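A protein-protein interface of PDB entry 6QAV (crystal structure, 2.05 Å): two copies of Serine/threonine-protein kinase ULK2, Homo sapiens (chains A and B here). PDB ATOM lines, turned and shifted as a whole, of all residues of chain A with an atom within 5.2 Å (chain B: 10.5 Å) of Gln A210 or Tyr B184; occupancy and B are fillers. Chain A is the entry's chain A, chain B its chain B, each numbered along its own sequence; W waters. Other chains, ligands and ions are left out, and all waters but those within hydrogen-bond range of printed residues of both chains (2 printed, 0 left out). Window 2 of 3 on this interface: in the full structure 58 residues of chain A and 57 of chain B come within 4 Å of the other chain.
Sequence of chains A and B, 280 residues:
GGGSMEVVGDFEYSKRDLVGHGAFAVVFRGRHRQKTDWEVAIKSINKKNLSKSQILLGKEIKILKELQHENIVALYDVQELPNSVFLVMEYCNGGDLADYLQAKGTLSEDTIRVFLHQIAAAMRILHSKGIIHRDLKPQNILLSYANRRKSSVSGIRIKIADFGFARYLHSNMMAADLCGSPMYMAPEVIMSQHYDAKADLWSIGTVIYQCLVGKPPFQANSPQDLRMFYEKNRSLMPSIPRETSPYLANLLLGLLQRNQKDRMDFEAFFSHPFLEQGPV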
ATOM      1  N   LEU A 101      -2.926  28.441 -34.205  1.00  0.00           N
ATOM      2  CA  LEU A 101      -3.923  27.367 -34.405  1.00  0.00           C
ATOM      3  C   LEU A 101      -4.625  27.556 -35.749  1.00  0.00           C
ATOM      4  O   LEU A 101      -4.949  26.583 -36.403  1.00  0.00           O
ATOM      5  CB  LEU A 101      -4.937  27.338 -33.257  1.00  0.00           C
ATOM      6  CG  LEU A 101      -4.378  26.939 -31.891  1.00  0.00           C
ATOM      7  CD1 LEU A 101      -5.473  26.859 -30.848  1.00  0.00           C
ATOM      8  CD2 LEU A 101      -3.621  25.641 -31.956  1.00  0.00           C
ATOM      9  N   GLY A 105      -4.195  24.197 -37.457  1.00  0.00           N
ATOM     10  CA  GLY A 105      -5.424  23.429 -37.320  1.00  0.00           C
ATOM     11  C   GLY A 105      -5.550  22.824 -35.931  1.00  0.00           C
ATOM     12  O   GLY A 105      -6.243  23.378 -35.045  1.00  0.00           O
ATOM     13  N   THR A 106      -4.892  21.679 -35.739  1.00  0.00           N
ATOM     14  CA  THR A 106      -4.690  21.090 -34.421  1.00  0.00           C
ATOM     15  C   THR A 106      -3.214  20.753 -34.292  1.00  0.00           C
ATOM     16  O   THR A 106      -2.519  20.631 -35.292  1.00  0.00           O
ATOM     17  CB  THR A 106      -5.525  19.819 -34.219  1.00  0.00           C
ATOM     18  OG1 THR A 106      -5.135  18.904 -35.227  1.00  0.00           O
ATOM     19  CG2 THR A 106      -7.010  20.023 -34.336  1.00  0.00           C
ATOM     20  N   LEU A 136      -6.677  33.643 -18.956  1.00  0.00           N
ATOM     21  CA  LEU A 136      -5.796  32.954 -19.898  1.00  0.00           C
ATOM     22  C   LEU A 136      -6.624  32.470 -21.075  1.00  0.00           C
ATOM     23  O   LEU A 136      -7.643  31.812 -20.879  1.00  0.00           O
ATOM     24  CB  LEU A 136      -5.135  31.745 -19.245  1.00  0.00           C
ATOM     25  CG  LEU A 136      -3.949  32.047 -18.349  1.00  0.00           C
ATOM     26  CD1 LEU A 136      -3.446  30.792 -17.678  1.00  0.00           C
ATOM     27  CD2 LEU A 136      -2.829  32.740 -19.131  1.00  0.00           C
ATOM     28  N   LYS A 137      -6.074  32.626 -22.277  1.00  0.00           N
ATOM     29  CA  LYS A 137      -6.763  32.228 -23.477  1.00  0.00           C
ATOM     30  C   LYS A 137      -5.803  32.260 -24.649  1.00  0.00           C
ATOM     31  O   LYS A 137      -4.700  32.798 -24.525  1.00  0.00           O
ATOM     32  CB  LYS A 137      -7.970  33.132 -23.684  1.00  0.00           C
ATOM     33  CG  LYS A 137      -7.668  34.618 -23.805  1.00  0.00           C
ATOM     34  CD  LYS A 137      -8.932  35.447 -23.905  1.00  0.00           C
ATOM     35  CE  LYS A 137      -8.660  36.934 -23.843  1.00  0.00           C
ATOM     36  NZ  LYS A 137      -9.914  37.698 -23.648  1.00  0.00           N
ATOM     37  N   PRO A 138      -6.167  31.681 -25.824  1.00  0.00           N
ATOM     38  CA  PRO A 138      -5.244  31.654 -26.963  1.00  0.00           C
ATOM     39  C   PRO A 138      -4.772  33.062 -27.378  1.00  0.00           C
ATOM     40  O   PRO A 138      -3.664  33.192 -27.858  1.00  0.00           O
ATOM     41  CB  PRO A 138      -6.035  30.916 -28.053  1.00  0.00           C
ATOM     42  CG  PRO A 138      -7.012  30.056 -27.269  1.00  0.00           C
ATOM     43  CD  PRO A 138      -7.404  30.930 -26.083  1.00  0.00           C
ATOM     44  N   GLN A 139      -5.587  34.094 -27.104  1.00  0.00           N
ATOM     45  CA  GLN A 139      -5.322  35.460 -27.569  1.00  0.00           C
ATOM     46  C   GLN A 139      -4.264  36.150 -26.694  1.00  0.00           C
ATOM     47  O   GLN A 139      -3.746  37.172 -27.100  1.00  0.00           O
ATOM     48  CB  GLN A 139      -6.620  36.285 -27.564  1.00  0.00           C
ATOM     49  CG  GLN A 139      -7.615  35.901 -28.670  1.00  0.00           C
ATOM     50  CD  GLN A 139      -8.357  34.591 -28.437  1.00  0.00           C
ATOM     51  OE1 GLN A 139      -8.524  34.095 -27.297  1.00  0.00           O
ATOM     52  NE2 GLN A 139      -8.805  33.998 -29.535  1.00  0.00           N
ATOM     53  N   TRP A 202      -8.253  25.683 -14.947  1.00  0.00           N
ATOM     54  CA  TRP A 202      -9.375  25.425 -15.854  1.00  0.00           C
ATOM     55  C   TRP A 202      -9.058  26.009 -17.230  1.00  0.00           C
ATOM     56  O   TRP A 202      -9.257  25.314 -18.248  1.00  0.00           O
ATOM     57  CB  TRP A 202     -10.694  25.987 -15.330  1.00  0.00           C
ATOM     58  CG  TRP A 202     -11.793  26.003 -16.357  1.00  0.00           C
ATOM     59  CD1 TRP A 202     -12.021  26.963 -17.297  1.00  0.00           C
ATOM     60  CD2 TRP A 202     -12.817  25.008 -16.557  1.00  0.00           C
ATOM     61  NE1 TRP A 202     -13.093  26.635 -18.077  1.00  0.00           N
ATOM     62  CE2 TRP A 202     -13.616  25.447 -17.639  1.00  0.00           C
ATOM     63  CE3 TRP A 202     -13.150  23.810 -15.921  1.00  0.00           C
ATOM     64  CZ2 TRP A 202     -14.723  24.731 -18.097  1.00  0.00           C
ATOM     65  CZ3 TRP A 202     -14.246  23.092 -16.365  1.00  0.00           C
ATOM     66  CH2 TRP A 202     -15.027  23.551 -17.438  1.00  0.00           C
ATOM     67  N   SER A 203      -8.654  27.301 -17.257  1.00  0.00           N
ATOM     68  CA  SER A 203      -8.379  27.959 -18.509  1.00  0.00           C
ATOM     69  C   SER A 203      -7.383  27.104 -19.330  1.00  0.00           C
ATOM     70  O   SER A 203      -7.598  26.858 -20.509  1.00  0.00           O
ATOM     71  CB  SER A 203      -7.902  29.389 -18.284  1.00  0.00           C
ATOM     72  OG  SER A 203      -8.840  30.119 -17.484  1.00  0.00           O
ATOM     73  N   GLY A 205      -6.690  24.051 -19.194  1.00  0.00           N
ATOM     74  CA  GLY A 205      -7.455  22.950 -19.663  1.00  0.00           C
ATOM     75  C   GLY A 205      -8.132  23.229 -20.993  1.00  0.00           C
ATOM     76  O   GLY A 205      -8.009  22.448 -21.945  1.00  0.00           O
ATOM     77  N   THR A 206      -8.873  24.327 -21.058  1.00  0.00           N
ATOM     78  CA  THR A 206      -9.652  24.656 -22.259  1.00  0.00           C
ATOM     79  C   THR A 206      -8.716  24.943 -23.438  1.00  0.00           C
ATOM     80  O   THR A 206      -9.058  24.646 -24.582  1.00  0.00           O
ATOM     81  CB  THR A 206     -10.596  25.846 -22.036  1.00  0.00           C
ATOM     82  OG1 THR A 206      -9.869  27.048 -21.753  1.00  0.00           O
ATOM     83  CG2 THR A 206     -11.567  25.583 -20.916  1.00  0.00           C
ATOM     84  N   VAL A 207      -7.549  25.535 -23.164  1.00  0.00           N
ATOM     85  CA  VAL A 207      -6.617  25.904 -24.219  1.00  0.00           C
ATOM     86  C   VAL A 207      -6.004  24.626 -24.801  1.00  0.00           C
ATOM     87  O   VAL A 207      -5.888  24.506 -26.018  1.00  0.00           O
ATOM     88  CB  VAL A 207      -5.530  26.871 -23.699  1.00  0.00           C
ATOM     89  CG1 VAL A 207      -4.371  27.026 -24.663  1.00  0.00           C
ATOM     90  CG2 VAL A 207      -6.125  28.205 -23.351  1.00  0.00           C
ATOM     91  N   ILE A 208      -5.561  23.717 -23.923  1.00  0.00           N
ATOM     92  CA  ILE A 208      -4.964  22.449 -24.358  1.00  0.00           C
ATOM     93  C   ILE A 208      -6.001  21.706 -25.216  1.00  0.00           C
ATOM     94  O   ILE A 208      -5.683  21.157 -26.268  1.00  0.00           O
ATOM     95  CB  ILE A 208      -4.553  21.577 -23.158  1.00  0.00           C
ATOM     96  CG1 ILE A 208      -3.472  22.221 -22.297  1.00  0.00           C
ATOM     97  CG2 ILE A 208      -4.148  20.175 -23.596  1.00  0.00           C
ATOM     98  CD1 ILE A 208      -3.345  21.551 -20.916  1.00  0.00           C
ATOM     99  N   TYR A 209      -7.246  21.653 -24.713  1.00  0.00           N
ATOM    100  CA  TYR A 209      -8.331  20.995 -25.427  1.00  0.00           C
ATOM    101  C   TYR A 209      -8.437  21.577 -26.843  1.00  0.00           C
ATOM    102  O   TYR A 209      -8.496  20.842 -27.823  1.00  0.00           O
ATOM    103  CB  TYR A 209      -9.655  21.129 -24.673  1.00  0.00           C
ATOM    104  CG  TYR A 209     -10.798  20.380 -25.310  1.00  0.00           C
ATOM    105  CD1 TYR A 209     -11.502  20.913 -26.378  1.00  0.00           C
ATOM    106  CD2 TYR A 209     -11.132  19.102 -24.878  1.00  0.00           C
ATOM    107  CE1 TYR A 209     -12.521  20.204 -26.984  1.00  0.00           C
ATOM    108  CE2 TYR A 209     -12.119  18.367 -25.499  1.00  0.00           C
ATOM    109  CZ  TYR A 209     -12.817  18.918 -26.558  1.00  0.00           C
ATOM    110  OH  TYR A 209     -13.843  18.234 -27.138  1.00  0.00           O
ATOM    111  N   GLN A 210      -8.447  22.913 -26.948  1.00  0.00           N
ATOM    112  CA  GLN A 210      -8.610  23.517 -28.231  1.00  0.00           C
ATOM    113  C   GLN A 210      -7.412  23.190 -29.126  1.00  0.00           C
ATOM    114  O   GLN A 210      -7.591  22.889 -30.298  1.00  0.00           O
ATOM    115  CB  GLN A 210      -8.814  25.021 -28.134  1.00  0.00           C
ATOM    116  CG  GLN A 210      -9.002  25.655 -29.506  1.00  0.00           C
ATOM    117  CD  GLN A 210      -9.378  27.104 -29.381  1.00  0.00           C
ATOM    118  OE1 GLN A 210      -9.818  27.576 -28.328  1.00  0.00           O
ATOM    119  NE2 GLN A 210      -9.151  27.842 -30.447  1.00  0.00           N
ATOM    120  N   CYS A 211      -6.197  23.212 -28.579  1.00  0.00           N
ATOM    121  CA  CYS A 211      -5.027  22.805 -29.349  1.00  0.00           C
ATOM    122  C   CYS A 211      -5.208  21.384 -29.934  1.00  0.00           C
ATOM    123  O   CYS A 211      -4.834  21.129 -31.099  1.00  0.00           O
ATOM    124  CB  CYS A 211      -3.771  22.836 -28.494  1.00  0.00           C
ATOM    125  SG  CYS A 211      -3.231  24.518 -28.051  1.00  0.00           S
ATOM    126  N   LEU A 212      -5.759  20.468 -29.133  1.00  0.00           N
ATOM    127  CA  LEU A 212      -5.853  19.026 -29.490  1.00  0.00           C
ATOM    128  C   LEU A 212      -6.997  18.789 -30.490  1.00  0.00           C
ATOM    129  O   LEU A 212      -6.819  18.121 -31.462  1.00  0.00           O
ATOM    130  CB  LEU A 212      -6.068  18.221 -28.206  1.00  0.00           C
ATOM    131  CG  LEU A 212      -6.239  16.714 -28.352  1.00  0.00           C
ATOM    132  CD1 LEU A 212      -4.946  16.057 -28.821  1.00  0.00           C
ATOM    133  CD2 LEU A 212      -6.673  16.124 -27.028  1.00  0.00           C
ATOM    134  N   VAL A 213      -8.139  19.441 -30.268  1.00  0.00           N
ATOM    135  CA  VAL A 213      -9.395  19.102 -30.943  1.00  0.00           C
ATOM    136  C   VAL A 213      -9.759  20.136 -32.018  1.00  0.00           C
ATOM    137  O   VAL A 213     -10.474  19.812 -32.956  1.00  0.00           O
ATOM    138  CB  VAL A 213     -10.513  18.974 -29.907  1.00  0.00           C
ATOM    139  CG1 VAL A 213     -11.860  18.660 -30.549  1.00  0.00           C
ATOM    140  CG2 VAL A 213     -10.148  17.938 -28.855  1.00  0.00           C
ATOM    141  N   GLY A 214      -9.358  21.391 -31.819  1.00  0.00           N
ATOM    142  CA  GLY A 214      -9.537  22.431 -32.834  1.00  0.00           C
ATOM    143  C   GLY A 214     -10.720  23.342 -32.565  1.00  0.00           C
ATOM    144  O   GLY A 214     -11.003  24.230 -33.357  1.00  0.00           O
ATOM    145  N   LYS A 215     -11.421  23.096 -31.454  1.00  0.00           N
ATOM    146  CA  LYS A 215     -12.418  23.996 -30.914  1.00  0.00           C
ATOM    147  C   LYS A 215     -12.314  23.963 -29.389  1.00  0.00           C
ATOM    148  O   LYS A 215     -11.741  23.034 -28.815  1.00  0.00           O
ATOM    149  CB  LYS A 215     -13.848  23.578 -31.306  1.00  0.00           C
ATOM    150  CG  LYS A 215     -14.041  22.990 -32.698  1.00  0.00           C
ATOM    151  CD  LYS A 215     -15.272  22.115 -32.840  1.00  0.00           C
ATOM    152  CE  LYS A 215     -15.416  21.563 -34.247  1.00  0.00           C
ATOM    153  NZ  LYS A 215     -16.836  21.482 -34.710  1.00  0.00           N
ATOM    154  N   PRO A 216     -12.934  24.937 -28.692  1.00  0.00           N
ATOM    155  CA  PRO A 216     -13.053  24.898 -27.239  1.00  0.00           C
ATOM    156  C   PRO A 216     -13.919  23.734 -26.790  1.00  0.00           C
ATOM    157  O   PRO A 216     -14.764  23.279 -27.556  1.00  0.00           O
ATOM    158  CB  PRO A 216     -13.756  26.210 -26.876  1.00  0.00           C
ATOM    159  CG  PRO A 216     -13.605  27.094 -28.112  1.00  0.00           C
ATOM    160  CD  PRO A 216     -13.536  26.144 -29.279  1.00  0.00           C
ATOM    161  N   PRO A 217     -13.771  23.224 -25.542  1.00  0.00           N
ATOM    162  CA  PRO A 217     -14.592  22.102 -25.090  1.00  0.00           C
ATOM    163  C   PRO A 217     -16.091  22.416 -24.958  1.00  0.00           C
ATOM    164  O   PRO A 217     -16.902  21.510 -25.036  1.00  0.00           O
ATOM    165  CB  PRO A 217     -13.989  21.709 -23.732  1.00  0.00           C
ATOM    166  CG  PRO A 217     -13.240  22.951 -23.280  1.00  0.00           C
ATOM    167  CD  PRO A 217     -12.772  23.644 -24.544  1.00  0.00           C
ATOM    168  N   ALA B 176     -16.374  39.425 -19.214  1.00  0.00           N
ATOM    169  CA  ALA B 176     -16.571  38.266 -20.097  1.00  0.00           C
ATOM    170  C   ALA B 176     -17.403  38.661 -21.329  1.00  0.00           C
ATOM    171  O   ALA B 176     -17.041  38.304 -22.457  1.00  0.00           O
ATOM    172  CB  ALA B 176     -17.217  37.138 -19.326  1.00  0.00           C
ATOM    173  N   CYS B 179     -15.306  40.621 -23.664  1.00  0.00           N
ATOM    174  CA  CYS B 179     -14.321  39.730 -24.311  1.00  0.00           C
ATOM    175  C   CYS B 179     -14.851  39.233 -25.667  1.00  0.00           C
ATOM    176  O   CYS B 179     -14.112  39.196 -26.651  1.00  0.00           O
ATOM    177  CB  CYS B 179     -14.040  38.498 -23.452  1.00  0.00           C
ATOM    178  SG  CYS B 179     -12.724  38.706 -22.231  1.00  0.00           S
ATOM    179  N   GLY B 180     -16.116  38.793 -25.679  1.00  0.00           N
ATOM    180  CA  GLY B 180     -16.691  38.047 -26.791  1.00  0.00           C
ATOM    181  C   GLY B 180     -16.408  36.554 -26.672  1.00  0.00           C
ATOM    182  O   GLY B 180     -17.303  35.735 -26.916  1.00  0.00           O
ATOM    183  N   SER B 181     -15.166  36.198 -26.280  1.00  0.00           N
ATOM    184  CA  SER B 181     -14.829  34.829 -25.779  1.00  0.00           C
ATOM    185  C   SER B 181     -14.764  34.801 -24.248  1.00  0.00           C
ATOM    186  O   SER B 181     -13.733  35.149 -23.665  1.00  0.00           O
ATOM    187  CB  SER B 181     -13.529  34.341 -26.360  1.00  0.00           C
ATOM    188  OG  SER B 181     -13.651  34.119 -27.756  1.00  0.00           O
ATOM    189  N   PRO B 182     -15.842  34.351 -23.552  1.00  0.00           N
ATOM    190  CA  PRO B 182     -15.793  34.025 -22.123  1.00  0.00           C
ATOM    191  C   PRO B 182     -15.442  32.537 -21.913  1.00  0.00           C
ATOM    192  O   PRO B 182     -15.632  31.968 -20.845  1.00  0.00           O
ATOM    193  CB  PRO B 182     -17.240  34.310 -21.694  1.00  0.00           C
ATOM    194  CG  PRO B 182     -18.077  33.927 -22.907  1.00  0.00           C
ATOM    195  CD  PRO B 182     -17.180  34.102 -24.117  1.00  0.00           C
ATOM    196  N   MET B 183     -14.939  31.927 -22.978  1.00  0.00           N
ATOM    197  CA  MET B 183     -14.983  30.518 -23.250  1.00  0.00           C
ATOM    198  C   MET B 183     -13.885  29.770 -22.480  1.00  0.00           C
ATOM    199  O   MET B 183     -13.893  28.542 -22.402  1.00  0.00           O
ATOM    200  CB  MET B 183     -14.744  30.355 -24.755  1.00  0.00           C
ATOM    201  CG  MET B 183     -15.275  29.116 -25.336  1.00  0.00           C
ATOM    202  SD  MET B 183     -15.873  29.492 -27.015  1.00  0.00           S
ATOM    203  CE  MET B 183     -17.447  30.268 -26.642  1.00  0.00           C
ATOM    204  N   TYR B 184     -12.899  30.524 -21.972  1.00  0.00           N
ATOM    205  CA  TYR B 184     -11.676  30.012 -21.393  1.00  0.00           C
ATOM    206  C   TYR B 184     -11.630  30.431 -19.937  1.00  0.00           C
ATOM    207  O   TYR B 184     -10.748  30.016 -19.167  1.00  0.00           O
ATOM    208  CB  TYR B 184     -10.462  30.519 -22.173  1.00  0.00           C
ATOM    209  CG  TYR B 184     -10.527  30.290 -23.662  1.00  0.00           C
ATOM    210  CD1 TYR B 184     -10.092  29.113 -24.223  1.00  0.00           C
ATOM    211  CD2 TYR B 184     -11.008  31.265 -24.516  1.00  0.00           C
ATOM    212  CE1 TYR B 184     -10.167  28.888 -25.584  1.00  0.00           C
ATOM    213  CE2 TYR B 184     -11.087  31.062 -25.881  1.00  0.00           C
ATOM    214  CZ  TYR B 184     -10.663  29.872 -26.423  1.00  0.00           C
ATOM    215  OH  TYR B 184     -10.734  29.647 -27.778  1.00  0.00           O
ATOM    216  N   MET B 185     -12.602  31.243 -19.539  1.00  0.00           N
ATOM    217  CA  MET B 185     -12.656  31.748 -18.181  1.00  0.00           C
ATOM    218  C   MET B 185     -13.163  30.601 -17.282  1.00  0.00           C
ATOM    219  O   MET B 185     -13.994  29.845 -17.690  1.00  0.00           O
ATOM    220  CB  MET B 185     -13.593  32.958 -18.102  1.00  0.00           C
ATOM    221  CG  MET B 185     -13.248  33.935 -17.020  1.00  0.00           C
ATOM    222  SD  MET B 185     -14.047  35.582 -17.293  1.00  0.00           S
ATOM    223  CE  MET B 185     -12.854  36.410 -18.345  1.00  0.00           C
ATOM    224  N   ALA B 186     -12.660  30.534 -16.047  1.00  0.00           N
ATOM    225  CA  ALA B 186     -13.051  29.507 -15.090  1.00  0.00           C
ATOM    226  C   ALA B 186     -14.513  29.704 -14.685  1.00  0.00           C
ATOM    227  O   ALA B 186     -14.964  30.830 -14.465  1.00  0.00           O
ATOM    228  CB  ALA B 186     -12.127  29.528 -13.882  1.00  0.00           C
ATOM    229  N   PRO B 187     -15.306  28.615 -14.533  1.00  0.00           N
ATOM    230  CA  PRO B 187     -16.679  28.728 -14.043  1.00  0.00           C
ATOM    231  C   PRO B 187     -16.816  29.600 -12.791  1.00  0.00           C
ATOM    232  O   PRO B 187     -17.677  30.464 -12.769  1.00  0.00           O
ATOM    233  CB  PRO B 187     -17.049  27.271 -13.761  1.00  0.00           C
ATOM    234  CG  PRO B 187     -16.278  26.519 -14.837  1.00  0.00           C
ATOM    235  CD  PRO B 187     -14.939  27.228 -14.859  1.00  0.00           C
ATOM    236  N   GLU B 188     -15.937  29.419 -11.804  1.00  0.00           N
ATOM    237  CA  GLU B 188     -16.045  30.163 -10.553  1.00  0.00           C
ATOM    238  C   GLU B 188     -15.769  31.668 -10.768  1.00  0.00           C
ATOM    239  O   GLU B 188     -16.142  32.489  -9.917  1.00  0.00           O
ATOM    240  CB  GLU B 188     -15.134  29.599  -9.464  1.00  0.00           C
ATOM    241  CG  GLU B 188     -13.652  29.713  -9.765  1.00  0.00           C
ATOM    242  CD  GLU B 188     -13.038  28.528 -10.487  1.00  0.00           C
ATOM    243  OE1 GLU B 188     -11.857  28.272 -10.247  1.00  0.00           O
ATOM    244  OE2 GLU B 188     -13.767  27.855 -11.251  1.00  0.00           O
ATOM    245  N   VAL B 189     -15.113  32.042 -11.879  1.00  0.00           N
ATOM    246  CA  VAL B 189     -14.888  33.469 -12.193  1.00  0.00           C
ATOM    247  C   VAL B 189     -16.154  34.036 -12.846  1.00  0.00           C
ATOM    248  O   VAL B 189     -16.667  35.067 -12.387  1.00  0.00           O
ATOM    249  CB  VAL B 189     -13.639  33.670 -13.070  1.00  0.00           C
ATOM    250  CG1 VAL B 189     -13.519  35.090 -13.604  1.00  0.00           C
ATOM    251  CG2 VAL B 189     -12.375  33.288 -12.317  1.00  0.00           C
ATOM    252  N   ILE B 190     -16.677  33.328 -13.857  1.00  0.00           N
ATOM    253  CA  ILE B 190     -17.928  33.666 -14.547  1.00  0.00           C
ATOM    254  C   ILE B 190     -19.093  33.853 -13.541  1.00  0.00           C
ATOM    255  O   ILE B 190     -20.000  34.675 -13.765  1.00  0.00           O
ATOM    256  CB  ILE B 190     -18.269  32.575 -15.584  1.00  0.00           C
ATOM    257  CG1 ILE B 190     -17.366  32.638 -16.817  1.00  0.00           C
ATOM    258  CG2 ILE B 190     -19.745  32.618 -15.963  1.00  0.00           C
ATOM    259  CD1 ILE B 190     -17.547  33.863 -17.676  1.00  0.00           C
HETATM  260  O   HOH W   1     -10.309  32.115 -15.351  1.00  0.00           O
HETATM  261  O   HOH W   2      -9.354  31.034 -30.428  1.00  0.00           O
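The side-chain amino group (NZ) of Lys A137 is in hydrogen-bond range of the side-chain sulfur (SG) of Cys B179 (3.3 Å).
The backbone carbonyl oxygen (O) of Met B185 lies within hydrogen-bond range of the indole nitrogen (NE1) of Trp A202, 3.4 Å away.
O of Tyr B184 lies within hydrogen-bond range of OG of Ser A203, at 2.5 Å.
OE1 of Gln A210 lies close to OH of Tyr B184.
The side-chain hydroxyl (OG1) of Thr A206 sits at hydrogen-bond distance from the backbone carbonyl oxygen (O) of Ser A203 (2.6 Å).
Among the printed residues, merely in contact across the chains: Leu A136 with Tyr B184, Lys A137 with Tyr B184, Pro A138 with Tyr B184, Trp A202 with Tyr B184, Trp A202 with Ala B186, Trp A202 with Pro B187, Thr A206 with Tyr B184, Pro A216 with Met B183 and Pro A216 with Tyr B184.
Of the printed residues of chain B, Leu A136 touches Tyr B184.
Printed residues of chain B within 4 Å of Lys A137: Cys B179 and Tyr B184.
Of the printed residues of chain B, Pro A138 touches Tyr B184 (3.4 Å).
Of chain B, only Tyr B184 (2.5 Å) comes within 4 Å of Ser A203.
Printed residues of chain B within 4 Å of Gln A210: Tyr B184.
No residue of chain B comes within 4 Å of Cys A211.
No residue of chain B comes within 4 Å of Val A213.
No residue of chain B comes within 4 Å of Gly A214.
Pro A216 touches just these residues of chain B: Met B183 and Tyr B184.
Gly B180 touches none of the printed residues of chain A.
Printed residues of chain A within 4 Å of Met B183: Pro A216 (3.5 Å).
Tyr B184 touches eight residues of chain A.
Of the printed residues of chain A, Ala B186 touches Trp A202 (3.5 Å).
The nearest residue of chain B that does not touch Gln A210 is Met B183 (6.4 Å).
The nearest printed residue of chain A that does not touch Pro B187 is Ser A203 (6.7 Å).
Hydrophobic or aromatic side chains of chain A that line the printed part of chain B: Pro A138, Trp A202 and Pro A216.
Hydrophobic or aromatic side chains of chain B that line the printed part of chain A: Met B183, Tyr B184 and Pro B187.
Along chain B the printed residues that touch a printed residue of chain A span positions 179 to 187.
Among the printed residues, 13 pairs touch across the chains.
No position is printed for both chains.
Water W1 bridges the backbone NH (N) of Ala B186 and the side-chain hydroxyl (OG) of Ser A203.
Water W2 lies within hydrogen-bond range of the side-chain amide nitrogen (NE2) of Gln A139 (3.1 Å), the side-chain amide nitrogen (NE2) of Gln A210 (3.2 Å) and the side-chain hydroxyl (OH) of Tyr B184 (3.3 Å).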
